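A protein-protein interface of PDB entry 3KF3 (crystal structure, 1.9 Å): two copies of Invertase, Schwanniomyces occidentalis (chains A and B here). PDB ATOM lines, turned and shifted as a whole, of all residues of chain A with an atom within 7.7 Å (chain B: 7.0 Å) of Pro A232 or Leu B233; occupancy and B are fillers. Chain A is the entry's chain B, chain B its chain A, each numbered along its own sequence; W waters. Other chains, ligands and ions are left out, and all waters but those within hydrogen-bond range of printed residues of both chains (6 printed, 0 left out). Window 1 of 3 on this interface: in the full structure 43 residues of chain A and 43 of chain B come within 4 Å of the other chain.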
ATOM      1  N   TYR A 198     -11.235  33.258 -29.094  1.00  0.00           N
ATOM      2  CA  TYR A 198     -10.608  31.949 -29.168  1.00  0.00           C
ATOM      3  C   TYR A 198     -11.655  30.875 -29.439  1.00  0.00           C
ATOM      4  O   TYR A 198     -12.541  30.644 -28.614  1.00  0.00           O
ATOM      5  CB  TYR A 198      -9.852  31.637 -27.870  1.00  0.00           C
ATOM      6  CG  TYR A 198      -8.650  30.753 -28.091  1.00  0.00           C
ATOM      7  CD1 TYR A 198      -7.428  31.308 -28.468  1.00  0.00           C
ATOM      8  CD2 TYR A 198      -8.728  29.368 -27.942  1.00  0.00           C
ATOM      9  CE1 TYR A 198      -6.316  30.522 -28.686  1.00  0.00           C
ATOM     10  CE2 TYR A 198      -7.604  28.558 -28.163  1.00  0.00           C
ATOM     11  CZ  TYR A 198      -6.400  29.153 -28.530  1.00  0.00           C
ATOM     12  OH  TYR A 198      -5.268  28.404 -28.752  1.00  0.00           O
ATOM     13  N   TYR A 199     -11.547  30.215 -30.589  1.00  0.00           N
ATOM     14  CA  TYR A 199     -12.567  29.253 -31.012  1.00  0.00           C
ATOM     15  C   TYR A 199     -12.481  27.934 -30.276  1.00  0.00           C
ATOM     16  O   TYR A 199     -13.507  27.385 -29.872  1.00  0.00           O
ATOM     17  CB  TYR A 199     -12.470  28.964 -32.510  1.00  0.00           C
ATOM     18  CG  TYR A 199     -13.086  30.000 -33.418  1.00  0.00           C
ATOM     19  CD1 TYR A 199     -13.367  31.289 -32.966  1.00  0.00           C
ATOM     20  CD2 TYR A 199     -13.358  29.697 -34.757  1.00  0.00           C
ATOM     21  CE1 TYR A 199     -13.922  32.236 -33.811  1.00  0.00           C
ATOM     22  CE2 TYR A 199     -13.912  30.644 -35.614  1.00  0.00           C
ATOM     23  CZ  TYR A 199     -14.188  31.905 -35.140  1.00  0.00           C
ATOM     24  OH  TYR A 199     -14.730  32.846 -35.982  1.00  0.00           O
ATOM     25  N   GLY A 200     -11.261  27.409 -30.141  1.00  0.00           N
ATOM     26  CA  GLY A 200     -11.069  26.033 -29.694  1.00  0.00           C
ATOM     27  C   GLY A 200     -11.917  25.075 -30.515  1.00  0.00           C
ATOM     28  O   GLY A 200     -12.081  25.250 -31.732  1.00  0.00           O
ATOM     29  N   ILE A 227     -15.660  27.859 -23.941  1.00  0.00           N
ATOM     30  CA  ILE A 227     -15.151  26.948 -24.965  1.00  0.00           C
ATOM     31  C   ILE A 227     -14.535  25.686 -24.349  1.00  0.00           C
ATOM     32  O   ILE A 227     -13.832  25.756 -23.344  1.00  0.00           O
ATOM     33  CB  ILE A 227     -14.142  27.622 -25.950  1.00  0.00           C
ATOM     34  CG1 ILE A 227     -12.926  28.191 -25.212  1.00  0.00           C
ATOM     35  CG2 ILE A 227     -14.835  28.701 -26.795  1.00  0.00           C
ATOM     36  CD1 ILE A 227     -11.650  28.254 -26.059  1.00  0.00           C
ATOM     37  N   PRO A 229     -13.396  21.396 -25.871  1.00  0.00           N
ATOM     38  CA  PRO A 229     -12.025  21.553 -25.384  1.00  0.00           C
ATOM     39  C   PRO A 229     -11.280  22.582 -26.248  1.00  0.00           C
ATOM     40  O   PRO A 229     -11.922  23.337 -26.996  1.00  0.00           O
ATOM     41  CB  PRO A 229     -11.443  20.141 -25.534  1.00  0.00           C
ATOM     42  CG  PRO A 229     -12.199  19.566 -26.715  1.00  0.00           C
ATOM     43  CD  PRO A 229     -13.591  20.122 -26.590  1.00  0.00           C
ATOM     44  N   GLY A 230      -9.954  22.630 -26.135  1.00  0.00           N
ATOM     45  CA  GLY A 230      -9.151  23.544 -26.947  1.00  0.00           C
ATOM     46  C   GLY A 230      -8.865  24.897 -26.324  1.00  0.00           C
ATOM     47  O   GLY A 230      -8.467  25.831 -27.023  1.00  0.00           O
ATOM     48  N   SER A 231      -9.056  25.013 -25.010  1.00  0.00           N
ATOM     49  CA  SER A 231      -8.559  26.180 -24.272  1.00  0.00           C
ATOM     50  C   SER A 231      -7.046  26.255 -24.445  1.00  0.00           C
ATOM     51  O   SER A 231      -6.378  25.223 -24.426  1.00  0.00           O
ATOM     52  CB  SER A 231      -8.891  26.051 -22.784  1.00  0.00           C
ATOM     53  OG  SER A 231      -8.196  27.019 -22.010  1.00  0.00           O
ATOM     54  N   PRO A 232      -6.488  27.473 -24.586  1.00  0.00           N
ATOM     55  CA  PRO A 232      -5.032  27.530 -24.685  1.00  0.00           C
ATOM     56  C   PRO A 232      -4.339  27.080 -23.394  1.00  0.00           C
ATOM     57  O   PRO A 232      -3.139  26.833 -23.398  1.00  0.00           O
ATOM     58  CB  PRO A 232      -4.760  29.009 -24.974  1.00  0.00           C
ATOM     59  CG  PRO A 232      -5.914  29.716 -24.417  1.00  0.00           C
ATOM     60  CD  PRO A 232      -7.091  28.815 -24.642  1.00  0.00           C
ATOM     61  N   LEU A 233      -5.099  26.963 -22.308  1.00  0.00           N
ATOM     62  CA  LEU A 233      -4.571  26.447 -21.050  1.00  0.00           C
ATOM     63  C   LEU A 233      -4.818  24.947 -20.928  1.00  0.00           C
ATOM     64  O   LEU A 233      -4.380  24.307 -19.964  1.00  0.00           O
ATOM     65  CB  LEU A 233      -5.211  27.184 -19.871  1.00  0.00           C
ATOM     66  CG  LEU A 233      -4.647  28.548 -19.457  1.00  0.00           C
ATOM     67  CD1 LEU A 233      -4.833  29.601 -20.540  1.00  0.00           C
ATOM     68  CD2 LEU A 233      -5.325  28.999 -18.173  1.00  0.00           C
ATOM     69  N   GLY A 234      -5.514  24.388 -21.915  1.00  0.00           N
ATOM     70  CA  GLY A 234      -5.843  22.973 -21.918  1.00  0.00           C
ATOM     71  C   GLY A 234      -7.241  22.761 -21.379  1.00  0.00           C
ATOM     72  O   GLY A 234      -7.559  23.184 -20.261  1.00  0.00           O
ATOM     73  N   GLY A 235      -8.082  22.130 -22.194  1.00  0.00           N
ATOM     74  CA  GLY A 235      -9.460  21.829 -21.807  1.00  0.00           C
ATOM     75  C   GLY A 235     -10.432  22.984 -21.970  1.00  0.00           C
ATOM     76  O   GLY A 235     -10.613  23.510 -23.080  1.00  0.00           O
ATOM     77  N   SER A 236     -11.047  23.370 -20.853  1.00  0.00           N
ATOM     78  CA  SER A 236     -12.178  24.291 -20.829  1.00  0.00           C
ATOM     79  C   SER A 236     -11.837  25.646 -20.208  1.00  0.00           C
ATOM     80  O   SER A 236     -11.033  25.730 -19.280  1.00  0.00           O
ATOM     81  CB  SER A 236     -13.338  23.653 -20.051  1.00  0.00           C
ATOM     82  OG  SER A 236     -12.886  23.083 -18.833  1.00  0.00           O
ATOM     83  N   ILE A 237     -12.479  26.695 -20.717  1.00  0.00           N
ATOM     84  CA  ILE A 237     -12.229  28.055 -20.254  1.00  0.00           C
ATOM     85  C   ILE A 237     -13.365  28.990 -20.665  1.00  0.00           C
ATOM     86  O   ILE A 237     -14.112  28.709 -21.624  1.00  0.00           O
ATOM     87  CB  ILE A 237     -10.852  28.583 -20.772  1.00  0.00           C
ATOM     88  CG1 ILE A 237     -10.261  29.617 -19.803  1.00  0.00           C
ATOM     89  CG2 ILE A 237     -10.966  29.099 -22.223  1.00  0.00           C
ATOM     90  CD1 ILE A 237      -8.807  29.949 -20.032  1.00  0.00           C
ATOM     91  N   GLN A 239     -14.305  33.047 -21.766  1.00  0.00           N
ATOM     92  CA  GLN A 239     -13.775  34.278 -22.311  1.00  0.00           C
ATOM     93  C   GLN A 239     -14.898  35.298 -22.390  1.00  0.00           C
ATOM     94  O   GLN A 239     -16.074  34.956 -22.204  1.00  0.00           O
ATOM     95  CB  GLN A 239     -13.152  34.047 -23.693  1.00  0.00           C
ATOM     96  CG  GLN A 239     -14.151  33.666 -24.784  1.00  0.00           C
ATOM     97  CD  GLN A 239     -13.456  33.238 -26.062  1.00  0.00           C
ATOM     98  OE1 GLN A 239     -12.784  34.035 -26.715  1.00  0.00           O
ATOM     99  NE2 GLN A 239     -13.602  31.968 -26.415  1.00  0.00           N
ATOM    100  N   THR A 257      -9.163  39.158 -27.596  1.00  0.00           N
ATOM    101  CA  THR A 257      -9.569  37.971 -26.852  1.00  0.00           C
ATOM    102  C   THR A 257      -9.101  38.100 -25.407  1.00  0.00           C
ATOM    103  O   THR A 257      -7.928  38.375 -25.156  1.00  0.00           O
ATOM    104  CB  THR A 257      -8.941  36.703 -27.482  1.00  0.00           C
ATOM    105  OG1 THR A 257      -9.571  36.446 -28.743  1.00  0.00           O
ATOM    106  CG2 THR A 257      -9.108  35.477 -26.577  1.00  0.00           C
ATOM    107  N   PHE A 259      -9.793  36.198 -21.330  1.00  0.00           N
ATOM    108  CA  PHE A 259     -10.417  35.133 -20.548  1.00  0.00           C
ATOM    109  C   PHE A 259     -10.969  35.664 -19.235  1.00  0.00           C
ATOM    110  O   PHE A 259     -10.423  36.597 -18.667  1.00  0.00           O
ATOM    111  CB  PHE A 259      -9.426  33.989 -20.333  1.00  0.00           C
ATOM    112  CG  PHE A 259      -8.987  33.347 -21.615  1.00  0.00           C
ATOM    113  CD1 PHE A 259      -7.669  33.454 -22.055  1.00  0.00           C
ATOM    114  CD2 PHE A 259      -9.911  32.685 -22.418  1.00  0.00           C
ATOM    115  CE1 PHE A 259      -7.275  32.876 -23.257  1.00  0.00           C
ATOM    116  CE2 PHE A 259      -9.529  32.108 -23.619  1.00  0.00           C
ATOM    117  CZ  PHE A 259      -8.211  32.204 -24.041  1.00  0.00           C
ATOM    118  N   LYS A 264      -7.314  26.936 -14.200  1.00  0.00           N
ATOM    119  CA  LYS A 264      -7.706  25.800 -15.008  1.00  0.00           C
ATOM    120  C   LYS A 264      -9.191  25.446 -14.839  1.00  0.00           C
ATOM    121  O   LYS A 264      -9.788  24.808 -15.710  1.00  0.00           O
ATOM    122  CB  LYS A 264      -6.835  24.604 -14.627  1.00  0.00           C
ATOM    123  CG  LYS A 264      -6.729  23.561 -15.692  1.00  0.00           C
ATOM    124  CD  LYS A 264      -5.487  23.744 -16.546  1.00  0.00           C
ATOM    125  CE  LYS A 264      -5.163  22.412 -17.168  1.00  0.00           C
ATOM    126  NZ  LYS A 264      -5.505  22.300 -18.592  1.00  0.00           N
ATOM    127  N   LYS A 432       1.524  24.384 -12.650  1.00  0.00           N
ATOM    128  CA  LYS A 432       2.077  25.740 -12.555  1.00  0.00           C
ATOM    129  C   LYS A 432       1.344  26.680 -13.497  1.00  0.00           C
ATOM    130  O   LYS A 432       1.219  26.395 -14.683  1.00  0.00           O
ATOM    131  CB  LYS A 432       3.584  25.752 -12.854  1.00  0.00           C
ATOM    132  CG  LYS A 432       4.438  24.954 -11.861  1.00  0.00           C
ATOM    133  CD  LYS A 432       5.899  24.899 -12.321  1.00  0.00           C
ATOM    134  CE  LYS A 432       6.741  24.010 -11.411  1.00  0.00           C
ATOM    135  NZ  LYS A 432       8.191  24.333 -11.560  1.00  0.00           N
ATOM    136  N   LEU A 433       0.841  27.786 -12.950  1.00  0.00           N
ATOM    137  CA  LEU A 433       0.120  28.793 -13.733  1.00  0.00           C
ATOM    138  C   LEU A 433       0.558  30.164 -13.248  1.00  0.00           C
ATOM    139  O   LEU A 433       0.852  30.340 -12.059  1.00  0.00           O
ATOM    140  CB  LEU A 433      -1.395  28.637 -13.556  1.00  0.00           C
ATOM    141  CG  LEU A 433      -2.085  27.343 -14.012  1.00  0.00           C
ATOM    142  CD1 LEU A 433      -3.470  27.236 -13.416  1.00  0.00           C
ATOM    143  CD2 LEU A 433      -2.162  27.293 -15.529  1.00  0.00           C
ATOM    144  N   ALA A 434       0.597  31.132 -14.160  1.00  0.00           N
ATOM    145  CA  ALA A 434       1.072  32.472 -13.832  1.00  0.00           C
ATOM    146  C   ALA A 434       0.094  33.554 -14.283  1.00  0.00           C
ATOM    147  O   ALA A 434      -0.797  33.301 -15.096  1.00  0.00           O
ATOM    148  CB  ALA A 434       2.440  32.702 -14.451  1.00  0.00           C
ATOM    149  N   TYR B 198      -4.814  38.352 -29.064  1.00  0.00           N
ATOM    150  CA  TYR B 198      -4.487  38.397 -27.644  1.00  0.00           C
ATOM    151  C   TYR B 198      -3.479  39.515 -27.430  1.00  0.00           C
ATOM    152  O   TYR B 198      -2.396  39.490 -28.011  1.00  0.00           O
ATOM    153  CB  TYR B 198      -3.914  37.053 -27.181  1.00  0.00           C
ATOM    154  CG  TYR B 198      -4.189  36.739 -25.732  1.00  0.00           C
ATOM    155  CD1 TYR B 198      -5.403  36.177 -25.345  1.00  0.00           C
ATOM    156  CD2 TYR B 198      -3.235  36.996 -24.742  1.00  0.00           C
ATOM    157  CE1 TYR B 198      -5.669  35.873 -24.006  1.00  0.00           C
ATOM    158  CE2 TYR B 198      -3.495  36.700 -23.391  1.00  0.00           C
ATOM    159  CZ  TYR B 198      -4.715  36.136 -23.038  1.00  0.00           C
ATOM    160  OH  TYR B 198      -4.996  35.833 -21.723  1.00  0.00           O
ATOM    161  N   GLY B 230       2.455  38.226 -20.784  1.00  0.00           N
ATOM    162  CA  GLY B 230       0.998  38.172 -20.896  1.00  0.00           C
ATOM    163  C   GLY B 230       0.450  37.099 -21.818  1.00  0.00           C
ATOM    164  O   GLY B 230      -0.746  37.083 -22.109  1.00  0.00           O
ATOM    165  N   SER B 231       1.306  36.187 -22.273  1.00  0.00           N
ATOM    166  CA  SER B 231       0.834  35.028 -23.027  1.00  0.00           C
ATOM    167  C   SER B 231      -0.134  34.221 -22.150  1.00  0.00           C
ATOM    168  O   SER B 231       0.078  34.124 -20.930  1.00  0.00           O
ATOM    169  CB  SER B 231       2.014  34.159 -23.448  1.00  0.00           C
ATOM    170  OG  SER B 231       1.611  32.838 -23.761  1.00  0.00           O
ATOM    171  N   PRO B 232      -1.196  33.642 -22.753  1.00  0.00           N
ATOM    172  CA  PRO B 232      -2.087  32.832 -21.917  1.00  0.00           C
ATOM    173  C   PRO B 232      -1.353  31.633 -21.316  1.00  0.00           C
ATOM    174  O   PRO B 232      -1.790  31.097 -20.304  1.00  0.00           O
ATOM    175  CB  PRO B 232      -3.178  32.354 -22.889  1.00  0.00           C
ATOM    176  CG  PRO B 232      -3.011  33.144 -24.123  1.00  0.00           C
ATOM    177  CD  PRO B 232      -1.599  33.624 -24.174  1.00  0.00           C
ATOM    178  N   LEU B 233      -0.242  31.228 -21.929  1.00  0.00           N
ATOM    179  CA  LEU B 233       0.577  30.128 -21.408  1.00  0.00           C
ATOM    180  C   LEU B 233       1.648  30.631 -20.440  1.00  0.00           C
ATOM    181  O   LEU B 233       2.413  29.843 -19.879  1.00  0.00           O
ATOM    182  CB  LEU B 233       1.226  29.345 -22.557  1.00  0.00           C
ATOM    183  CG  LEU B 233       0.309  28.435 -23.388  1.00  0.00           C
ATOM    184  CD1 LEU B 233      -0.757  29.229 -24.164  1.00  0.00           C
ATOM    185  CD2 LEU B 233       1.147  27.600 -24.336  1.00  0.00           C
ATOM    186  N   GLY B 234       1.693  31.947 -20.246  1.00  0.00           N
ATOM    187  CA  GLY B 234       2.671  32.570 -19.365  1.00  0.00           C
ATOM    188  C   GLY B 234       3.875  33.020 -20.168  1.00  0.00           C
ATOM    189  O   GLY B 234       4.481  32.233 -20.878  1.00  0.00           O
ATOM    190  N   GLY B 235       4.201  34.302 -20.085  1.00  0.00           N
ATOM    191  CA  GLY B 235       5.394  34.823 -20.747  1.00  0.00           C
ATOM    192  C   GLY B 235       5.145  35.208 -22.189  1.00  0.00           C
ATOM    193  O   GLY B 235       4.256  36.014 -22.484  1.00  0.00           O
ATOM    194  N   SER B 236       5.910  34.584 -23.081  1.00  0.00           N
ATOM    195  CA  SER B 236       6.036  34.988 -24.475  1.00  0.00           C
ATOM    196  C   SER B 236       5.407  33.978 -25.429  1.00  0.00           C
ATOM    197  O   SER B 236       5.484  32.762 -25.203  1.00  0.00           O
ATOM    198  CB  SER B 236       7.519  35.183 -24.810  1.00  0.00           C
ATOM    199  OG  SER B 236       8.300  34.066 -24.394  1.00  0.00           O
ATOM    200  N   ILE B 237       4.781  34.485 -26.494  1.00  0.00           N
ATOM    201  CA  ILE B 237       4.141  33.624 -27.495  1.00  0.00           C
ATOM    202  C   ILE B 237       3.919  34.356 -28.821  1.00  0.00           C
ATOM    203  O   ILE B 237       3.841  35.588 -28.848  1.00  0.00           O
ATOM    204  CB  ILE B 237       2.788  33.050 -26.951  1.00  0.00           C
ATOM    205  CG1 ILE B 237       2.423  31.733 -27.648  1.00  0.00           C
ATOM    206  CG2 ILE B 237       1.678  34.094 -27.036  1.00  0.00           C
ATOM    207  CD1 ILE B 237       1.354  30.908 -26.909  1.00  0.00           C
ATOM    208  N   PHE B 259      -2.664  30.843 -32.072  1.00  0.00           N
ATOM    209  CA  PHE B 259      -1.228  30.861 -31.828  1.00  0.00           C
ATOM    210  C   PHE B 259      -0.464  30.035 -32.853  1.00  0.00           C
ATOM    211  O   PHE B 259      -0.979  29.038 -33.369  1.00  0.00           O
ATOM    212  CB  PHE B 259      -0.916  30.457 -30.376  1.00  0.00           C
ATOM    213  CG  PHE B 259      -1.544  31.376 -29.368  1.00  0.00           C
ATOM    214  CD1 PHE B 259      -2.610  30.954 -28.576  1.00  0.00           C
ATOM    215  CD2 PHE B 259      -1.107  32.691 -29.257  1.00  0.00           C
ATOM    216  CE1 PHE B 259      -3.215  31.829 -27.661  1.00  0.00           C
ATOM    217  CE2 PHE B 259      -1.703  33.578 -28.355  1.00  0.00           C
ATOM    218  CZ  PHE B 259      -2.753  33.144 -27.553  1.00  0.00           C
ATOM    219  N   ASP B 261       2.541  28.506 -32.293  1.00  0.00           N
ATOM    220  CA  ASP B 261       3.117  27.344 -31.628  1.00  0.00           C
ATOM    221  C   ASP B 261       2.629  27.371 -30.195  1.00  0.00           C
ATOM    222  O   ASP B 261       2.708  28.399 -29.523  1.00  0.00           O
ATOM    223  CB  ASP B 261       4.647  27.398 -31.701  1.00  0.00           C
ATOM    224  CG  ASP B 261       5.323  26.165 -31.108  1.00  0.00           C
ATOM    225  OD1 ASP B 261       5.173  25.917 -29.884  1.00  0.00           O
ATOM    226  OD2 ASP B 261       6.030  25.449 -31.868  1.00  0.00           O
ATOM    227  N   ILE B 262       2.105  26.248 -29.728  1.00  0.00           N
ATOM    228  CA  ILE B 262       1.469  26.227 -28.418  1.00  0.00           C
ATOM    229  C   ILE B 262       2.340  25.512 -27.386  1.00  0.00           C
ATOM    230  O   ILE B 262       1.849  24.972 -26.393  1.00  0.00           O
ATOM    231  CB  ILE B 262       0.014  25.686 -28.471  1.00  0.00           C
ATOM    232  CG1 ILE B 262      -0.036  24.288 -29.102  1.00  0.00           C
ATOM    233  CG2 ILE B 262      -0.899  26.690 -29.210  1.00  0.00           C
ATOM    234  CD1 ILE B 262      -1.306  23.525 -28.767  1.00  0.00           C
ATOM    235  N   GLY B 263       3.647  25.533 -27.635  1.00  0.00           N
ATOM    236  CA  GLY B 263       4.615  25.216 -26.603  1.00  0.00           C
ATOM    237  C   GLY B 263       4.967  26.490 -25.854  1.00  0.00           C
ATOM    238  O   GLY B 263       4.484  27.579 -26.175  1.00  0.00           O
ATOM    239  N   LYS B 264       5.816  26.361 -24.847  1.00  0.00           N
ATOM    240  CA  LYS B 264       6.238  27.526 -24.090  1.00  0.00           C
ATOM    241  C   LYS B 264       7.337  28.334 -24.797  1.00  0.00           C
ATOM    242  O   LYS B 264       7.491  29.538 -24.556  1.00  0.00           O
ATOM    243  CB  LYS B 264       6.740  27.068 -22.735  1.00  0.00           C
ATOM    244  CG  LYS B 264       6.731  28.146 -21.715  1.00  0.00           C
ATOM    245  CD  LYS B 264       5.466  28.148 -20.875  1.00  0.00           C
ATOM    246  CE  LYS B 264       5.858  28.824 -19.587  1.00  0.00           C
ATOM    247  NZ  LYS B 264       4.766  29.571 -18.973  1.00  0.00           N
ATOM    248  N   ASN B 287      11.582  31.195 -23.679  1.00  0.00           N
ATOM    249  CA  ASN B 287      10.506  32.018 -23.163  1.00  0.00           C
ATOM    250  C   ASN B 287      11.153  33.063 -22.262  1.00  0.00           C
ATOM    251  O   ASN B 287      12.011  32.718 -21.437  1.00  0.00           O
ATOM    252  CB  ASN B 287       9.545  31.131 -22.361  1.00  0.00           C
ATOM    253  CG  ASN B 287       8.307  31.859 -21.907  1.00  0.00           C
ATOM    254  OD1 ASN B 287       8.379  32.876 -21.205  1.00  0.00           O
ATOM    255  ND2 ASN B 287       7.150  31.330 -22.289  1.00  0.00           N
ATOM    256  N   GLN B 289      10.297  34.419 -19.605  1.00  0.00           N
ATOM    257  CA  GLN B 289      10.139  34.162 -18.166  1.00  0.00           C
ATOM    258  C   GLN B 289      11.386  33.567 -17.532  1.00  0.00           C
ATOM    259  O   GLN B 289      11.706  33.868 -16.381  1.00  0.00           O
ATOM    260  CB  GLN B 289       8.975  33.208 -17.899  1.00  0.00           C
ATOM    261  CG  GLN B 289       7.601  33.823 -18.040  1.00  0.00           C
ATOM    262  CD  GLN B 289       6.515  32.788 -17.859  1.00  0.00           C
ATOM    263  OE1 GLN B 289       6.672  31.639 -18.269  1.00  0.00           O
ATOM    264  NE2 GLN B 289       5.412  33.182 -17.223  1.00  0.00           N
ATOM    265  N   PHE B 428       7.858  29.418 -13.291  1.00  0.00           N
ATOM    266  CA  PHE B 428       7.225  29.756 -14.561  1.00  0.00           C
ATOM    267  C   PHE B 428       7.507  28.699 -15.618  1.00  0.00           C
ATOM    268  O   PHE B 428       7.008  28.784 -16.734  1.00  0.00           O
ATOM    269  CB  PHE B 428       7.709  31.136 -15.024  1.00  0.00           C
ATOM    270  CG  PHE B 428       7.401  32.226 -14.045  1.00  0.00           C
ATOM    271  CD1 PHE B 428       8.410  32.785 -13.264  1.00  0.00           C
ATOM    272  CD2 PHE B 428       6.087  32.659 -13.862  1.00  0.00           C
ATOM    273  CE1 PHE B 428       8.117  33.784 -12.341  1.00  0.00           C
ATOM    274  CE2 PHE B 428       5.782  33.661 -12.938  1.00  0.00           C
ATOM    275  CZ  PHE B 428       6.798  34.226 -12.179  1.00  0.00           C
ATOM    276  N   THR B 430       6.561  25.820 -16.919  1.00  0.00           N
ATOM    277  CA  THR B 430       5.433  24.904 -17.000  1.00  0.00           C
ATOM    278  C   THR B 430       5.891  23.529 -17.500  1.00  0.00           C
ATOM    279  O   THR B 430       6.558  23.421 -18.529  1.00  0.00           O
ATOM    280  CB  THR B 430       4.346  25.472 -17.928  1.00  0.00           C
ATOM    281  OG1 THR B 430       4.155  26.867 -17.636  1.00  0.00           O
ATOM    282  CG2 THR B 430       3.024  24.708 -17.758  1.00  0.00           C
ATOM    283  N   LEU B 433       1.832  20.351 -20.694  1.00  0.00           N
ATOM    284  CA  LEU B 433       1.130  21.082 -21.747  1.00  0.00           C
ATOM    285  C   LEU B 433       0.383  20.080 -22.602  1.00  0.00           C
ATOM    286  O   LEU B 433       0.768  18.911 -22.670  1.00  0.00           O
ATOM    287  CB  LEU B 433       2.112  21.859 -22.629  1.00  0.00           C
ATOM    288  CG  LEU B 433       2.971  22.937 -21.960  1.00  0.00           C
ATOM    289  CD1 LEU B 433       4.237  23.194 -22.758  1.00  0.00           C
ATOM    290  CD2 LEU B 433       2.178  24.208 -21.789  1.00  0.00           C
ATOM    291  N   ALA B 434      -0.672  20.539 -23.263  1.00  0.00           N
ATOM    292  CA  ALA B 434      -1.509  19.658 -24.065  1.00  0.00           C
ATOM    293  C   ALA B 434      -1.902  20.312 -25.382  1.00  0.00           C
ATOM    294  O   ALA B 434      -1.754  21.530 -25.547  1.00  0.00           O
ATOM    295  CB  ALA B 434      -2.746  19.260 -23.273  1.00  0.00           C
HETATM  296  O   HOH W   1       0.929  30.473 -16.838  1.00  0.00           O
HETATM  297  O   HOH W   2      -0.398  33.632 -17.948  1.00  0.00           O
HETATM  298  O   HOH W   3      -7.005  36.870 -20.565  1.00  0.00           O
HETATM  299  O   HOH W   4      -4.143  23.289 -24.884  1.00  0.00           O
HETATM  300  O   HOH W   5       1.698  27.756 -16.921  1.00  0.00           O
HETATM  301  O   HOH W   6      -4.090  28.433 -31.095  1.00  0.00           O
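N of Leu B233 sits close to OG of Ser B231 (3.1 Å).
The backbone carbonyl oxygen of Leu B233 lies within hydrogen-bond range of the side-chain amino group of Lys B264 (2.5 Å).
The backbone carbonyl oxygen (O) of Phe B428 lies close to the side-chain amide oxygen (OE1) of Gln B289.
The backbone carbonyl oxygen (O) of Tyr A198 lies within hydrogen-bond range of the side-chain amide nitrogen (NE2) of Gln A239 (2.8 Å).
The side-chain hydroxyl of Ser A231 sits close to the backbone NH of Leu A233, 3.1 Å away.
The side-chain amino group (NZ) of Lys A264 lies within hydrogen-bond range of the backbone carbonyl oxygen (O) of Leu A233, 2.7 Å away.
CE1 of Tyr A198 touches CE1 of Phe B259 (3.5 Å).
Pro A232 touches Leu B233.
CD1 of Leu A233 touches O of Pro B232, at 3.4 Å.
Thr A257 touches Tyr B198.
CE1 of Phe A259 touches CE1 of Tyr B198, 3.5 Å away.
Thr B430 touches Lys A432 (CG2 to O, 3.9 Å).
CB of Ala A434 touches CD2 of Phe B428 (3.7 Å).
Printed residues of chain B within 4 Å of Pro A232: Leu B233.
Printed residues of chain A within 4 Å of Leu B233: Pro A232 (3.5 Å).
Of the printed residues of chain A, Pro B232 touches Leu A233 (3.4 Å).
Of the printed residues of chain B, Leu A233 touches Pro B232 (3.4 Å).
Printed residues of chain A within 4 Å of Phe B428: Ala A434 (3.7 Å).
Of the printed residues of chain B, Ala A434 touches Phe B428 (3.7 Å).
The nearest residue of chain B that does not touch Pro A232 is Pro B232 (4.1 Å).
The nearest residue of chain A that does not touch Leu B233 is Leu A233 (5.1 Å).
Hydrophobic or aromatic side chains of chain B that line the printed part of chain A: Tyr B198, Pro B232, Leu B233, Phe B259 and Phe B428.
Printed residues of chain A that touch a printed residue of chain B: Tyr A198, Pro A232, Leu A233, Thr A257, Phe A259, Lys A432 and Ala A434.
Hydrophobic or aromatic side chains of chain A that line the printed part of chain B: Tyr A198, Leu A233, Phe A259 and Ala A434.
Among the printed residues, no Asp or Glu carboxylate lies within 4 Å of a Lys or Arg side-chain nitrogen of the other chain.
Tyr A198 touches Phe B259, and with the chains exchanged Phe A259 touches Tyr B198.
Pro A232 touches Leu B233, and with the chains exchanged Leu A233 touches Pro B232.
13 positions are printed for both chains.
Of the 7 pairs that touch across the chains among the printed residues, 4 have their exchanged pair printed and touching as well.
Water W3 lies within hydrogen-bond range of the side-chain hydroxyl (OH) of Tyr B198 (2.5 Å) and the backbone NH (N) of Phe A259 (3.0 Å).
Water W6 bridges OH of Tyr A198 and N of Phe B259.
Water W5 bridges the backbone carbonyl oxygen (O) of Lys A432 (2.7 Å) and the side-chain hydroxyl (OG1) of Thr B430 (2.7 Å).
Water W1 lies within hydrogen-bond range of N of Ala A434 (2.8 Å) and O of Leu B233 (3.4 Å).
Water W2 bridges the backbone carbonyl oxygen (O) of Ala A434 (2.9 Å) and the backbone carbonyl oxygen (O) of Ser B231 (3.1 Å).
Water W4 lies within hydrogen-bond range of O of Ser A231 (3.0 Å), O of Ala B434 (3.0 Å) and N of Gly A234 (3.4 Å).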
